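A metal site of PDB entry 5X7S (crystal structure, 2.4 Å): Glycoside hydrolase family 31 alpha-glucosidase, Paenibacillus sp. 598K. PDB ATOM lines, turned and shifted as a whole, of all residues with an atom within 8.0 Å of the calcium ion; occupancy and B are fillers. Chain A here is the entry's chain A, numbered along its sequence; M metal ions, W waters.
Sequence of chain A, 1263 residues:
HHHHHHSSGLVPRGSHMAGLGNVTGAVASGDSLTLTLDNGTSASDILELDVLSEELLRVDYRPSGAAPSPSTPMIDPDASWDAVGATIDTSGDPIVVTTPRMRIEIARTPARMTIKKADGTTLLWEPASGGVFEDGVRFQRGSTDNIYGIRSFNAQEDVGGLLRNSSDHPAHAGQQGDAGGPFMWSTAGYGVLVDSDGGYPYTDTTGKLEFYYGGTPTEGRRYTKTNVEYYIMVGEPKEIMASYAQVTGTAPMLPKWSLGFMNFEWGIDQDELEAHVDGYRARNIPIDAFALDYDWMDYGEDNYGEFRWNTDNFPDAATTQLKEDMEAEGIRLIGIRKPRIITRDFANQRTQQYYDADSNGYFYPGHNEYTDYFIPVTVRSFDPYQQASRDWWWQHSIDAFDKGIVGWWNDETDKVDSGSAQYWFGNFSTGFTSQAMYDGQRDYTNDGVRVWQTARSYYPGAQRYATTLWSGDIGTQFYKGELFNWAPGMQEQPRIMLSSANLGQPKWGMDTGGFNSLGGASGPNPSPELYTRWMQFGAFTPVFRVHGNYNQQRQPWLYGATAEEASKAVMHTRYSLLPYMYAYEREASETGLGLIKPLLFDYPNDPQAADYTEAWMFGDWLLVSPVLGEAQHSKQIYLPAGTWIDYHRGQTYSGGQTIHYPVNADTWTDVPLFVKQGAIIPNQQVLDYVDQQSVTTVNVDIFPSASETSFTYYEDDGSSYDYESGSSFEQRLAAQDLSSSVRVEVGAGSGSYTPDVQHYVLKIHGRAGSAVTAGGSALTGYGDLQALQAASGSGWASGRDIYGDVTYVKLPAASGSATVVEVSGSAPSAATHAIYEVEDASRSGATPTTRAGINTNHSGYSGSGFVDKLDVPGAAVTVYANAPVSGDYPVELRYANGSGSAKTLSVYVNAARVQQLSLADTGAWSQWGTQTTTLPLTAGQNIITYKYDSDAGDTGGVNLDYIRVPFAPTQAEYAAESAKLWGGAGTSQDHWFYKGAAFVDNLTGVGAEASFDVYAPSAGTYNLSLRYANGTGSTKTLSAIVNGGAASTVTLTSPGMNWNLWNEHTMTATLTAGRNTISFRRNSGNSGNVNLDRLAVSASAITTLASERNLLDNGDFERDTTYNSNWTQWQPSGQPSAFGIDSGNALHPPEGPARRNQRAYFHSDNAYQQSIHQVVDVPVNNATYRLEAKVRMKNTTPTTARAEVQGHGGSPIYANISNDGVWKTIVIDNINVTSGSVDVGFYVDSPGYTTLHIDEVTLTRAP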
ATOM      1  N   THR A 562      35.035   9.828  11.617  1.00  0.00           N
ATOM      2  CA  THR A 562      36.365   9.785  12.253  1.00  0.00           C
ATOM      3  C   THR A 562      37.354   9.020  11.407  1.00  0.00           C
ATOM      4  O   THR A 562      38.436   9.513  11.078  1.00  0.00           O
ATOM      5  CB  THR A 562      36.373   9.195  13.665  1.00  0.00           C
ATOM      6  OG1 THR A 562      35.494   9.942  14.514  1.00  0.00           O
ATOM      7  CG2 THR A 562      37.760   9.270  14.263  1.00  0.00           C
ATOM      8  N   ASP A 666      39.000   9.869  22.378  1.00  0.00           N
ATOM      9  CA  ASP A 666      37.769  10.328  21.720  1.00  0.00           C
ATOM     10  C   ASP A 666      37.920  10.715  20.207  1.00  0.00           C
ATOM     11  O   ASP A 666      37.091  10.347  19.409  1.00  0.00           O
ATOM     12  CB  ASP A 666      37.134  11.458  22.530  1.00  0.00           C
ATOM     13  CG  ASP A 666      35.723  11.718  22.120  1.00  0.00           C
ATOM     14  OD1 ASP A 666      35.017  10.765  21.716  1.00  0.00           O
ATOM     15  OD2 ASP A 666      35.285  12.864  22.176  1.00  0.00           O
ATOM     16  N   ASN A1114      26.285   9.863  27.300  1.00  0.00           N
ATOM     17  CA  ASN A1114      26.409   8.889  26.250  1.00  0.00           C
ATOM     18  C   ASN A1114      25.605   9.245  24.983  1.00  0.00           C
ATOM     19  O   ASN A1114      24.997   8.394  24.327  1.00  0.00           O
ATOM     20  CB  ASN A1114      26.007   7.482  26.750  1.00  0.00           C
ATOM     21  CG  ASN A1114      26.608   6.374  25.898  1.00  0.00           C
ATOM     22  OD1 ASN A1114      27.677   6.542  25.283  1.00  0.00           O
ATOM     23  ND2 ASN A1114      25.906   5.264  25.801  1.00  0.00           N
ATOM     24  N   GLY A1115      25.633  10.520  24.617  1.00  0.00           N
ATOM     25  CA  GLY A1115      24.828  10.987  23.507  1.00  0.00           C
ATOM     26  C   GLY A1115      25.368  10.481  22.195  1.00  0.00           C
ATOM     27  O   GLY A1115      24.591  10.314  21.239  1.00  0.00           O
ATOM     28  N   ASP A1116      26.682  10.256  22.148  1.00  0.00           N
ATOM     29  CA  ASP A1116      27.371   9.616  20.995  1.00  0.00           C
ATOM     30  C   ASP A1116      27.352   8.058  21.034  1.00  0.00           C
ATOM     31  O   ASP A1116      27.935   7.420  20.151  1.00  0.00           O
ATOM     32  CB  ASP A1116      28.793  10.131  20.861  1.00  0.00           C
ATOM     33  CG  ASP A1116      29.591   9.986  22.151  1.00  0.00           C
ATOM     34  OD1 ASP A1116      29.141   9.212  23.067  1.00  0.00           O
ATOM     35  OD2 ASP A1116      30.646  10.641  22.237  1.00  0.00           O
ATOM     36  N   PHE A1117      26.695   7.457  22.046  1.00  0.00           N
ATOM     37  CA  PHE A1117      26.671   6.003  22.229  1.00  0.00           C
ATOM     38  C   PHE A1117      28.064   5.296  22.171  1.00  0.00           C
ATOM     39  O   PHE A1117      28.165   4.076  21.880  1.00  0.00           O
ATOM     40  CB  PHE A1117      25.714   5.391  21.218  1.00  0.00           C
ATOM     41  CG  PHE A1117      24.366   6.053  21.181  1.00  0.00           C
ATOM     42  CD1 PHE A1117      23.410   5.739  22.116  1.00  0.00           C
ATOM     43  CD2 PHE A1117      24.080   7.022  20.215  1.00  0.00           C
ATOM     44  CE1 PHE A1117      22.181   6.353  22.101  1.00  0.00           C
ATOM     45  CE2 PHE A1117      22.850   7.639  20.191  1.00  0.00           C
ATOM     46  CZ  PHE A1117      21.889   7.303  21.129  1.00  0.00           C
ATOM     47  N   GLU A1118      29.129   6.044  22.492  1.00  0.00           N
ATOM     48  CA  GLU A1118      30.491   5.498  22.430  1.00  0.00           C
ATOM     49  C   GLU A1118      30.866   4.642  23.640  1.00  0.00           C
ATOM     50  O   GLU A1118      31.856   3.927  23.592  1.00  0.00           O
ATOM     51  CB  GLU A1118      31.516   6.602  22.265  1.00  0.00           C
ATOM     52  CG  GLU A1118      31.390   7.263  20.925  1.00  0.00           C
ATOM     53  CD  GLU A1118      31.682   6.314  19.801  1.00  0.00           C
ATOM     54  OE1 GLU A1118      32.612   5.498  19.873  1.00  0.00           O
ATOM     55  OE2 GLU A1118      30.951   6.364  18.811  1.00  0.00           O
ATOM     56  N   ARG A1119      30.090   4.702  24.711  1.00  0.00           N
ATOM     57  CA  ARG A1119      30.409   3.942  25.908  1.00  0.00           C
ATOM     58  C   ARG A1119      30.335   2.491  25.533  1.00  0.00           C
ATOM     59  O   ARG A1119      29.487   2.088  24.723  1.00  0.00           O
ATOM     60  CB  ARG A1119      29.405   4.218  27.029  1.00  0.00           C
ATOM     61  CG  ARG A1119      29.725   3.476  28.330  1.00  0.00           C
ATOM     62  CD  ARG A1119      29.068   4.072  29.591  1.00  0.00           C
ATOM     63  NE  ARG A1119      29.194   5.523  29.630  1.00  0.00           N
ATOM     64  CZ  ARG A1119      28.248   6.390  30.038  1.00  0.00           C
ATOM     65  NH1 ARG A1119      27.074   5.984  30.504  1.00  0.00           N
ATOM     66  NH2 ARG A1119      28.479   7.672  29.983  1.00  0.00           N
ATOM     67  N   ILE A1141      23.123  -0.975  20.218  1.00  0.00           N
ATOM     68  CA  ILE A1141      24.255  -0.069  19.947  1.00  0.00           C
ATOM     69  C   ILE A1141      25.418  -0.924  19.465  1.00  0.00           C
ATOM     70  O   ILE A1141      25.757  -1.869  20.123  1.00  0.00           O
ATOM     71  CB  ILE A1141      24.684   0.650  21.238  1.00  0.00           C
ATOM     72  CG1 ILE A1141      23.550   1.560  21.758  1.00  0.00           C
ATOM     73  CG2 ILE A1141      25.962   1.456  21.022  1.00  0.00           C
ATOM     74  CD1 ILE A1141      23.596   1.805  23.273  1.00  0.00           C
ATOM     75  N   ASP A1142      25.988  -0.633  18.309  1.00  0.00           N
ATOM     76  CA  ASP A1142      27.213  -1.293  17.848  1.00  0.00           C
ATOM     77  C   ASP A1142      27.851  -0.460  16.708  1.00  0.00           C
ATOM     78  O   ASP A1142      27.399   0.638  16.396  1.00  0.00           O
ATOM     79  CB  ASP A1142      26.930  -2.774  17.431  1.00  0.00           C
ATOM     80  CG  ASP A1142      26.103  -2.903  16.109  1.00  0.00           C
ATOM     81  OD1 ASP A1142      26.094  -1.943  15.312  1.00  0.00           O
ATOM     82  OD2 ASP A1142      25.502  -3.986  15.850  1.00  0.00           O
ATOM     83  N   GLY A1152      28.740   2.294   8.996  1.00  0.00           N
ATOM     84  CA  GLY A1152      29.400   2.961  10.136  1.00  0.00           C
ATOM     85  C   GLY A1152      28.617   3.988  10.979  1.00  0.00           C
ATOM     86  O   GLY A1152      27.463   4.314  10.660  1.00  0.00           O
ATOM     87  N   PRO A1153      29.229   4.497  12.077  1.00  0.00           N
ATOM     88  CA  PRO A1153      28.564   5.511  12.902  1.00  0.00           C
ATOM     89  C   PRO A1153      28.821   6.855  12.247  1.00  0.00           C
ATOM     90  O   PRO A1153      29.636   6.910  11.320  1.00  0.00           O
ATOM     91  CB  PRO A1153      29.299   5.378  14.236  1.00  0.00           C
ATOM     92  CG  PRO A1153      30.705   5.053  13.833  1.00  0.00           C
ATOM     93  CD  PRO A1153      30.589   4.208  12.579  1.00  0.00           C
ATOM     94  N   ALA A1154      28.135   7.919  12.676  1.00  0.00           N
ATOM     95  CA  ALA A1154      28.485   9.259  12.190  1.00  0.00           C
ATOM     96  C   ALA A1154      29.858   9.729  12.686  1.00  0.00           C
ATOM     97  O   ALA A1154      30.590  10.407  11.940  1.00  0.00           O
ATOM     98  CB  ALA A1154      27.432  10.292  12.573  1.00  0.00           C
ATOM     99  N   ARG A1155      30.208   9.400  13.929  1.00  0.00           N
ATOM    100  CA  ARG A1155      31.533   9.735  14.477  1.00  0.00           C
ATOM    101  C   ARG A1155      32.063   8.622  15.395  1.00  0.00           C
ATOM    102  O   ARG A1155      31.287   7.975  16.147  1.00  0.00           O
ATOM    103  CB  ARG A1155      31.485  11.082  15.258  1.00  0.00           C
ATOM    104  CG  ARG A1155      32.818  11.828  15.409  1.00  0.00           C
ATOM    105  CD  ARG A1155      32.821  12.910  16.526  1.00  0.00           C
ATOM    106  NE  ARG A1155      32.601  12.339  17.862  1.00  0.00           N
ATOM    107  CZ  ARG A1155      33.552  11.777  18.622  1.00  0.00           C
ATOM    108  NH1 ARG A1155      34.834  11.722  18.223  1.00  0.00           N
ATOM    109  NH2 ARG A1155      33.187  11.256  19.790  1.00  0.00           N
ATOM    110  N   ARG A1156      33.377   8.436  15.363  1.00  0.00           N
ATOM    111  CA  ARG A1156      34.081   7.527  16.281  1.00  0.00           C
ATOM    112  C   ARG A1156      33.682   6.092  15.980  1.00  0.00           C
ATOM    113  O   ARG A1156      33.757   5.710  14.818  1.00  0.00           O
ATOM    114  CB  ARG A1156      33.924   7.934  17.760  1.00  0.00           C
ATOM    115  CG  ARG A1156      34.919   7.268  18.702  1.00  0.00           C
ATOM    116  CD  ARG A1156      34.946   7.834  20.111  1.00  0.00           C
ATOM    117  NE  ARG A1156      36.083   7.259  20.834  1.00  0.00           N
ATOM    118  CZ  ARG A1156      36.140   6.033  21.380  1.00  0.00           C
ATOM    119  NH1 ARG A1156      35.103   5.178  21.327  1.00  0.00           N
ATOM    120  NH2 ARG A1156      37.251   5.681  22.005  1.00  0.00           N
ATOM    121  N   ASN A1157      33.190   5.346  16.974  1.00  0.00           N
ATOM    122  CA  ASN A1157      33.099   3.901  16.890  1.00  0.00           C
ATOM    123  C   ASN A1157      31.722   3.283  16.876  1.00  0.00           C
ATOM    124  O   ASN A1157      31.559   2.274  16.220  1.00  0.00           O
ATOM    125  CB  ASN A1157      33.851   3.242  18.033  1.00  0.00           C
ATOM    126  CG  ASN A1157      34.412   1.906  17.605  1.00  0.00           C
ATOM    127  OD1 ASN A1157      34.922   1.758  16.479  1.00  0.00           O
ATOM    128  ND2 ASN A1157      34.328   0.919  18.488  1.00  0.00           N
ATOM    129  N   GLN A1158      30.740   3.859  17.568  1.00  0.00           N
ATOM    130  CA  GLN A1158      29.422   3.240  17.706  1.00  0.00           C
ATOM    131  C   GLN A1158      28.272   4.194  17.356  1.00  0.00           C
ATOM    132  O   GLN A1158      28.430   5.400  17.325  1.00  0.00           O
ATOM    133  CB  GLN A1158      29.259   2.671  19.123  1.00  0.00           C
ATOM    134  CG  GLN A1158      30.043   1.363  19.322  1.00  0.00           C
ATOM    135  CD  GLN A1158      30.157   0.869  20.755  1.00  0.00           C
ATOM    136  OE1 GLN A1158      30.553  -0.303  21.005  1.00  0.00           O
ATOM    137  NE2 GLN A1158      29.851   1.733  21.722  1.00  0.00           N
ATOM    138  N   ARG A1159      27.110   3.620  17.109  1.00  0.00           N
ATOM    139  CA  ARG A1159      25.869   4.377  16.933  1.00  0.00           C
ATOM    140  C   ARG A1159      24.733   3.502  17.376  1.00  0.00           C
ATOM    141  O   ARG A1159      24.782   2.280  17.197  1.00  0.00           O
ATOM    142  CB  ARG A1159      25.677   4.815  15.467  1.00  0.00           C
ATOM    143  CG  ARG A1159      25.295   3.727  14.433  1.00  0.00           C
ATOM    144  CD  ARG A1159      26.448   2.830  14.055  1.00  0.00           C
ATOM    145  NE  ARG A1159      26.106   1.857  13.004  1.00  0.00           N
ATOM    146  CZ  ARG A1159      25.418   0.732  13.168  1.00  0.00           C
ATOM    147  NH1 ARG A1159      24.945   0.370  14.362  1.00  0.00           N
ATOM    148  NH2 ARG A1159      25.208  -0.048  12.119  1.00  0.00           N
ATOM    149  N   ALA A1160      23.683   4.113  17.885  1.00  0.00           N
ATOM    150  CA  ALA A1160      22.502   3.333  18.207  1.00  0.00           C
ATOM    151  C   ALA A1160      21.840   2.917  16.902  1.00  0.00           C
ATOM    152  O   ALA A1160      22.077   3.519  15.852  1.00  0.00           O
ATOM    153  CB  ALA A1160      21.552   4.126  19.070  1.00  0.00           C
ATOM    154  N   TRP A1223      23.476  10.054   6.090  1.00  0.00           N
ATOM    155  CA  TRP A1223      23.558  10.792   7.331  1.00  0.00           C
ATOM    156  C   TRP A1223      23.036  12.194   7.104  1.00  0.00           C
ATOM    157  O   TRP A1223      23.551  12.895   6.230  1.00  0.00           O
ATOM    158  CB  TRP A1223      25.000  10.827   7.876  1.00  0.00           C
ATOM    159  CG  TRP A1223      25.423   9.553   8.609  1.00  0.00           C
ATOM    160  CD1 TRP A1223      26.414   8.729   8.233  1.00  0.00           C
ATOM    161  CD2 TRP A1223      24.846   8.964   9.819  1.00  0.00           C
ATOM    162  NE1 TRP A1223      26.527   7.678   9.124  1.00  0.00           N
ATOM    163  CE2 TRP A1223      25.569   7.793  10.107  1.00  0.00           C
ATOM    164  CE3 TRP A1223      23.819   9.346  10.703  1.00  0.00           C
ATOM    165  CZ2 TRP A1223      25.316   6.988  11.224  1.00  0.00           C
ATOM    166  CZ3 TRP A1223      23.567   8.538  11.830  1.00  0.00           C
ATOM    167  CH2 TRP A1223      24.293   7.373  12.066  1.00  0.00           C
ATOM    168  N   ILE A1254      21.104   6.335  14.818  1.00  0.00           N
ATOM    169  CA  ILE A1254      21.085   7.564  15.605  1.00  0.00           C
ATOM    170  C   ILE A1254      22.455   7.745  16.222  1.00  0.00           C
ATOM    171  O   ILE A1254      23.021   6.816  16.690  1.00  0.00           O
ATOM    172  CB  ILE A1254      20.108   7.446  16.784  1.00  0.00           C
ATOM    173  CG1 ILE A1254      18.702   7.070  16.293  1.00  0.00           C
ATOM    174  CG2 ILE A1254      20.061   8.748  17.569  1.00  0.00           C
ATOM    175  CD1 ILE A1254      17.822   6.539  17.430  1.00  0.00           C
ATOM    176  N   ASP A1255      22.952   8.970  16.266  1.00  0.00           N
ATOM    177  CA  ASP A1255      24.334   9.211  16.658  1.00  0.00           C
ATOM    178  C   ASP A1255      24.577  10.696  16.963  1.00  0.00           C
ATOM    179  O   ASP A1255      23.833  11.547  16.509  1.00  0.00           O
ATOM    180  CB  ASP A1255      25.299   8.704  15.576  1.00  0.00           C
ATOM    181  CG  ASP A1255      26.733   8.457  16.095  1.00  0.00           C
ATOM    182  OD1 ASP A1255      26.886   8.379  17.354  1.00  0.00           O
ATOM    183  OD2 ASP A1255      27.718   8.321  15.283  1.00  0.00           O
ATOM    184  N   GLU A1256      25.589  10.964  17.791  1.00  0.00           N
ATOM    185  CA  GLU A1256      26.128  12.297  18.061  1.00  0.00           C
ATOM    186  C   GLU A1256      25.013  13.197  18.532  1.00  0.00           C
ATOM    187  O   GLU A1256      24.859  14.323  18.069  1.00  0.00           O
ATOM    188  CB  GLU A1256      26.793  12.882  16.829  1.00  0.00           C
ATOM    189  CG  GLU A1256      28.067  12.161  16.415  1.00  0.00           C
ATOM    190  CD  GLU A1256      29.200  12.510  17.365  1.00  0.00           C
ATOM    191  OE1 GLU A1256      29.764  13.645  17.198  1.00  0.00           O
ATOM    192  OE2 GLU A1256      29.441  11.701  18.308  1.00  0.00           O
ATOM    193  N   VAL A1257      24.255  12.700  19.507  1.00  0.00           N
ATOM    194  CA  VAL A1257      23.140  13.465  20.058  1.00  0.00           C
ATOM    195  C   VAL A1257      23.703  14.418  21.097  1.00  0.00           C
ATOM    196  O   VAL A1257      24.384  13.971  22.014  1.00  0.00           O
ATOM    197  CB  VAL A1257      22.070  12.539  20.635  1.00  0.00           C
ATOM    198  CG1 VAL A1257      20.794  13.312  20.929  1.00  0.00           C
ATOM    199  CG2 VAL A1257      21.788  11.406  19.628  1.00  0.00           C
HETATM  200 CA    CA M   1      28.991   7.585  17.825  1.00  0.00          CA
HETATM  201  O   HOH W   1      30.289   9.422  17.690  1.00  0.00           O
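The side-chain carboxylate (OD2) of Asp 1255 is in hydrogen-bond range of the backbone NH (N) of Ala 1154, 2.7 Å away. NE2 of Gln 1158 is in hydrogen-bond range of O of Phe 1117, 2.9 Å away. The side-chain amide nitrogen of Gln 1158 lies within hydrogen-bond range of the backbone carbonyl oxygen of Arg 1119 (3.0 Å). The backbone NH (N) of Asn 1157 lies within hydrogen-bond range of the side-chain carboxylate (OE1) of Glu 1118 (3.0 Å). NH1 of Arg 1156 lies within salt-bridge range of OE1 of Glu 1118 (2.9 Å). The side-chain amide oxygen (OD1) of Asn 1114 sits at hydrogen-bond distance from the backbone NH (N) of Glu 1118. The side-chain carboxylate (OE1) of Glu 1256 is in salt-bridge range of the guanidinium group (NE) of Arg 1155 (3.2 Å). The guanidinium group (NH2) of Arg 1155 is in salt-bridge range of the side-chain carboxylate (OD1) of Asp 666.
Within 4 Å of the calcium ion: Asp 1116, Glu 1118, Arg 1155, Gln 1158 and Asp 1255. The nearest printed residue that does not touch the calcium ion is Glu 1256 (4.2 Å).
The calcium ion is bound by water W1 (2.3 Å), the side-chain carboxylate of Asp 1255 (2.3 Å), the backbone carbonyl oxygen of Gln 1158 (2.3 Å), the side-chain carboxylate of Glu 1118 (2.5 Å), the backbone carbonyl oxygen of Asp 1116 (2.6 Å) and the backbone carbonyl oxygen of Arg 1155 (2.9 Å). Slightly farther from the calcium ion lies the side-chain carboxylate (OD2) of Asp 1255 (2.9 Å).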
